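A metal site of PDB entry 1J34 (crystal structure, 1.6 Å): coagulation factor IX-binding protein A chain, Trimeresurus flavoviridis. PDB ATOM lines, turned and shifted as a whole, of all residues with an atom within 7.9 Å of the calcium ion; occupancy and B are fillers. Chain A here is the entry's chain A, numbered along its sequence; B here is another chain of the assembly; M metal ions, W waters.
The side-chain carboxylate (OE2) of Glu 128 lies close to the side-chain hydroxyl (OH) of Tyr 14 (3.3 Å).
OG of Ser 41 lies close to ND2 of Asn 81 of chain B (3.4 Å).
The side-chain carboxylate of Glu 47 sits close to the side-chain hydroxyl of Tyr 14, 2.7 Å away.
The backbone NH of Glu 47 is in hydrogen-bond range of the side-chain hydroxyl of Ser 44 (3.2 Å).
N of Glu 47 is in hydrogen-bond range of OH of Tyr 9, 3.4 Å away.
Within 4 Å of the calcium ion: Ser 41, Glu 43, Glu 47 and Glu 128.
The calcium ion is bound by the side-chain carboxylate (OE2) of Glu 128 (2.4 Å), the backbone carbonyl oxygen (O) of Ser 41 (2.4 Å), the side-chain carboxylate (OE2) of Glu 47 (2.4 Å), the side-chain carboxylate (OE2) of Glu 43 (2.4 Å), water W2 (2.4 Å), the side-chain hydroxyl (OG) of Ser 41 (2.5 Å), water W1 (2.5 Å) and the side-chain carboxylate (OE1) of Glu 128 (2.6 Å).
The calcium ion has eight donor atoms within binding distance.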
ATOM      1  N   TYR A   9      -1.114   8.745  16.092  1.00  0.00           N
ATOM      2  CA  TYR A   9      -1.173   7.323  15.736  1.00  0.00           C
ATOM      3  C   TYR A   9       0.200   6.861  15.285  1.00  0.00           C
ATOM      4  O   TYR A   9       0.757   7.364  14.309  1.00  0.00           O
ATOM      5  CB  TYR A   9      -2.182   7.048  14.624  1.00  0.00           C
ATOM      6  CG  TYR A   9      -2.259   5.572  14.279  1.00  0.00           C
ATOM      7  CD1 TYR A   9      -2.885   4.658  15.135  1.00  0.00           C
ATOM      8  CD2 TYR A   9      -1.680   5.065  13.110  1.00  0.00           C
ATOM      9  CE1 TYR A   9      -2.928   3.297  14.841  1.00  0.00           C
ATOM     10  CE2 TYR A   9      -1.711   3.705  12.809  1.00  0.00           C
ATOM     11  CZ  TYR A   9      -2.340   2.831  13.673  1.00  0.00           C
ATOM     12  OH  TYR A   9      -2.370   1.490  13.362  1.00  0.00           O
ATOM     13  N   GLU A  10       0.739   5.887  16.009  1.00  0.00           N
ATOM     14  CA  GLU A  10       2.040   5.299  15.730  1.00  0.00           C
ATOM     15  C   GLU A  10       3.103   6.297  15.255  1.00  0.00           C
ATOM     16  O   GLU A  10       3.607   6.184  14.130  1.00  0.00           O
ATOM     17  CB  GLU A  10       1.897   4.150  14.733  1.00  0.00           C
ATOM     18  CG  GLU A  10       0.933   3.053  15.189  1.00  0.00           C
ATOM     19  CD  GLU A  10       1.010   1.790  14.347  1.00  0.00           C
ATOM     20  OE1 GLU A  10       1.386   1.885  13.155  1.00  0.00           O
ATOM     21  OE2 GLU A  10       0.675   0.710  14.871  1.00  0.00           O
ATOM     22  N   HIS A  12       2.976   9.422  14.273  1.00  0.00           N
ATOM     23  CA  HIS A  12       2.598  10.550  13.423  1.00  0.00           C
ATOM     24  C   HIS A  12       1.384  11.310  13.937  1.00  0.00           C
ATOM     25  O   HIS A  12       0.663  10.821  14.807  1.00  0.00           O
ATOM     26  CB  HIS A  12       2.338  10.070  11.995  1.00  0.00           C
ATOM     27  CG  HIS A  12       3.569   9.578  11.291  1.00  0.00           C
ATOM     28  ND1 HIS A  12       4.670  10.378  11.091  1.00  0.00           N
ATOM     29  CD2 HIS A  12       3.869   8.379  10.748  1.00  0.00           C
ATOM     30  CE1 HIS A  12       5.608   9.691  10.453  1.00  0.00           C
ATOM     31  NE2 HIS A  12       5.143   8.477  10.239  1.00  0.00           N
ATOM     32  N   TYR A  14      -2.162  13.369  12.859  1.00  0.00           N
ATOM     33  CA  TYR A  14      -3.179  13.479  11.815  1.00  0.00           C
ATOM     34  C   TYR A  14      -4.225  14.522  12.149  1.00  0.00           C
ATOM     35  O   TYR A  14      -4.531  14.755  13.320  1.00  0.00           O
ATOM     36  CB  TYR A  14      -3.881  12.130  11.627  1.00  0.00           C
ATOM     37  CG  TYR A  14      -2.944  10.968  11.395  1.00  0.00           C
ATOM     38  CD1 TYR A  14      -2.124  10.489  12.420  1.00  0.00           C
ATOM     39  CD2 TYR A  14      -2.861  10.351  10.153  1.00  0.00           C
ATOM     40  CE1 TYR A  14      -1.245   9.426  12.205  1.00  0.00           C
ATOM     41  CE2 TYR A  14      -1.996   9.293   9.918  1.00  0.00           C
ATOM     42  CZ  TYR A  14      -1.190   8.827  10.947  1.00  0.00           C
ATOM     43  OH  TYR A  14      -0.329   7.790  10.731  1.00  0.00           O
ATOM     44  N   LEU A  39      -0.801  15.311   2.499  1.00  0.00           N
ATOM     45  CA  LEU A  39      -2.097  14.649   2.556  1.00  0.00           C
ATOM     46  C   LEU A  39      -1.746  13.321   3.184  1.00  0.00           C
ATOM     47  O   LEU A  39      -0.622  12.835   3.037  1.00  0.00           O
ATOM     48  CB  LEU A  39      -2.662  14.449   1.143  1.00  0.00           C
ATOM     49  CG  LEU A  39      -3.436  15.657   0.617  1.00  0.00           C
ATOM     50  CD1 LEU A  39      -3.737  15.495  -0.857  1.00  0.00           C
ATOM     51  CD2 LEU A  39      -4.739  15.799   1.417  1.00  0.00           C
ATOM     52  N   VAL A  40      -2.673  12.726   3.919  1.00  0.00           N
ATOM     53  CA  VAL A  40      -2.420  11.471   4.604  1.00  0.00           C
ATOM     54  C   VAL A  40      -1.923  10.343   3.705  1.00  0.00           C
ATOM     55  O   VAL A  40      -2.368  10.190   2.564  1.00  0.00           O
ATOM     56  CB  VAL A  40      -3.677  11.000   5.380  1.00  0.00           C
ATOM     57  CG1 VAL A  40      -4.774  10.587   4.417  1.00  0.00           C
ATOM     58  CG2 VAL A  40      -3.311   9.875   6.340  1.00  0.00           C
ATOM     59  N   SER A  41      -0.972   9.565   4.220  1.00  0.00           N
ATOM     60  CA  SER A  41      -0.418   8.423   3.496  1.00  0.00           C
ATOM     61  C   SER A  41      -0.827   7.165   4.269  1.00  0.00           C
ATOM     62  O   SER A  41      -0.377   6.947   5.388  1.00  0.00           O
ATOM     63  CB  SER A  41       1.107   8.529   3.397  1.00  0.00           C
ATOM     64  OG  SER A  41       1.712   8.656   4.677  1.00  0.00           O
ATOM     65  N   ILE A  42      -1.682   6.351   3.658  1.00  0.00           N
ATOM     66  CA  ILE A  42      -2.168   5.120   4.288  1.00  0.00           C
ATOM     67  C   ILE A  42      -1.216   3.969   3.964  1.00  0.00           C
ATOM     68  O   ILE A  42      -1.255   3.423   2.859  1.00  0.00           O
ATOM     69  CB  ILE A  42      -3.582   4.749   3.783  1.00  0.00           C
ATOM     70  CG1 ILE A  42      -4.501   5.971   3.860  1.00  0.00           C
ATOM     71  CG2 ILE A  42      -4.145   3.603   4.630  1.00  0.00           C
ATOM     72  CD1 ILE A  42      -4.715   6.509   5.251  1.00  0.00           C
ATOM     73  N   GLU A  43      -0.386   3.608   4.927  1.00  0.00           N
ATOM     74  CA  GLU A  43       0.619   2.559   4.738  1.00  0.00           C
ATOM     75  C   GLU A  43       0.390   1.240   5.460  1.00  0.00           C
ATOM     76  O   GLU A  43       1.256   0.366   5.459  1.00  0.00           O
ATOM     77  CB  GLU A  43       1.978   3.128   5.121  1.00  0.00           C
ATOM     78  CG  GLU A  43       2.284   4.423   4.412  1.00  0.00           C
ATOM     79  CD  GLU A  43       3.343   5.225   5.126  1.00  0.00           C
ATOM     80  OE1 GLU A  43       4.497   4.763   5.192  1.00  0.00           O
ATOM     81  OE2 GLU A  43       3.007   6.318   5.627  1.00  0.00           O
ATOM     82  N   SER A  44      -0.776   1.080   6.081  1.00  0.00           N
ATOM     83  CA  SER A  44      -1.104  -0.169   6.758  1.00  0.00           C
ATOM     84  C   SER A  44      -2.599  -0.199   7.045  1.00  0.00           C
ATOM     85  O   SER A  44      -3.254   0.843   7.021  1.00  0.00           O
ATOM     86  CB  SER A  44      -0.327  -0.314   8.066  1.00  0.00           C
ATOM     87  OG  SER A  44      -0.727   0.668   9.009  1.00  0.00           O
ATOM     88  N   GLU A  47      -3.452   1.844  10.137  1.00  0.00           N
ATOM     89  CA  GLU A  47      -3.455   3.281   9.884  1.00  0.00           C
ATOM     90  C   GLU A  47      -4.723   3.617   9.117  1.00  0.00           C
ATOM     91  O   GLU A  47      -5.348   4.653   9.358  1.00  0.00           O
ATOM     92  CB  GLU A  47      -2.208   3.687   9.080  1.00  0.00           C
ATOM     93  CG  GLU A  47      -2.146   5.174   8.748  1.00  0.00           C
ATOM     94  CD  GLU A  47      -0.831   5.569   8.098  1.00  0.00           C
ATOM     95  OE1 GLU A  47      -0.224   4.720   7.420  1.00  0.00           O
ATOM     96  OE2 GLU A  47      -0.416   6.741   8.262  1.00  0.00           O
ATOM     97  N   VAL A  51      -7.464   6.316  10.423  1.00  0.00           N
ATOM     98  CA  VAL A  51      -7.900   7.433   9.602  1.00  0.00           C
ATOM     99  C   VAL A  51      -9.407   7.381   9.343  1.00  0.00           C
ATOM    100  O   VAL A  51     -10.090   8.413   9.354  1.00  0.00           O
ATOM    101  CB  VAL A  51      -7.148   7.459   8.249  1.00  0.00           C
ATOM    102  CG1 VAL A  51      -7.739   8.533   7.332  1.00  0.00           C
ATOM    103  CG2 VAL A  51      -5.670   7.727   8.490  1.00  0.00           C
ATOM    104  N   GLU A 128      -1.262  14.688   7.351  1.00  0.00           N
ATOM    105  CA  GLU A 128      -0.447  13.861   8.224  1.00  0.00           C
ATOM    106  C   GLU A 128       0.964  14.430   8.315  1.00  0.00           C
ATOM    107  O   GLU A 128       1.507  14.921   7.316  1.00  0.00           O
ATOM    108  CB  GLU A 128      -0.372  12.420   7.698  1.00  0.00           C
ATOM    109  CG  GLU A 128       0.602  11.537   8.479  1.00  0.00           C
ATOM    110  CD  GLU A 128       0.740  10.136   7.893  1.00  0.00           C
ATOM    111  OE1 GLU A 128       0.080   9.832   6.876  1.00  0.00           O
ATOM    112  OE2 GLU A 128       1.519   9.336   8.455  1.00  0.00           O
ATOM    113  N   ALA A 129       1.542  14.383   9.501  1.00  0.00           N
ATOM    114  CA  ALA A 129       2.903  14.884   9.696  1.00  0.00           C
ATOM    115  C   ALA A 129       3.687  13.847  10.482  1.00  0.00           C
ATOM    116  O   ALA A 129       3.194  13.399  11.531  1.00  0.00           O
ATOM    117  CB  ALA A 129       2.879  16.202  10.440  1.00  0.00           C
ATOM    118  OXT ALA A 129       4.810  13.500  10.038  1.00  0.00           O
ATOM    119  N   TRP B  79       2.813   8.287  -3.238  1.00  0.00           N
ATOM    120  CA  TRP B  79       2.308   9.019  -2.083  1.00  0.00           C
ATOM    121  C   TRP B  79       3.016  10.369  -2.104  1.00  0.00           C
ATOM    122  O   TRP B  79       4.214  10.429  -2.379  1.00  0.00           O
ATOM    123  CB  TRP B  79       2.653   8.283  -0.778  1.00  0.00           C
ATOM    124  CG  TRP B  79       1.862   7.041  -0.535  1.00  0.00           C
ATOM    125  CD1 TRP B  79       2.305   5.755  -0.603  1.00  0.00           C
ATOM    126  CD2 TRP B  79       0.468   6.958  -0.198  1.00  0.00           C
ATOM    127  NE1 TRP B  79       1.288   4.872  -0.316  1.00  0.00           N
ATOM    128  CE2 TRP B  79       0.153   5.594  -0.067  1.00  0.00           C
ATOM    129  CE3 TRP B  79      -0.530   7.918   0.015  1.00  0.00           C
ATOM    130  CZ2 TRP B  79      -1.140   5.156   0.254  1.00  0.00           C
ATOM    131  CZ3 TRP B  79      -1.818   7.484   0.345  1.00  0.00           C
ATOM    132  CH2 TRP B  79      -2.101   6.113   0.458  1.00  0.00           C
ATOM    133  N   ASN B  81       4.106  12.097   0.208  1.00  0.00           N
ATOM    134  CA  ASN B  81       5.165  12.200   1.201  1.00  0.00           C
ATOM    135  C   ASN B  81       6.317  11.266   0.849  1.00  0.00           C
ATOM    136  O   ASN B  81       7.231  11.060   1.645  1.00  0.00           O
ATOM    137  CB  ASN B  81       4.635  11.864   2.594  1.00  0.00           C
ATOM    138  CG  ASN B  81       4.456  10.371   2.800  1.00  0.00           C
ATOM    139  OD1 ASN B  81       4.060   9.649   1.884  1.00  0.00           O
ATOM    140  ND2 ASN B  81       4.755   9.899   4.010  1.00  0.00           N
ATOM    141  N   ALA B  83       6.311   8.073   0.600  1.00  0.00           N
ATOM    142  CA  ALA B  83       6.305   6.785   1.289  1.00  0.00           C
ATOM    143  C   ALA B  83       6.213   5.673   0.255  1.00  0.00           C
ATOM    144  O   ALA B  83       5.602   5.846  -0.802  1.00  0.00           O
ATOM    145  CB  ALA B  83       5.115   6.708   2.247  1.00  0.00           C
HETATM  146 CA    CA M   1       1.371   7.570   6.879  1.00  0.00          CA
HETATM  147  O   HOH W   1       3.609   8.708   6.944  1.00  0.00           O
HETATM  148  O   HOH W   2       2.610   6.343   8.588  1.00  0.00           O
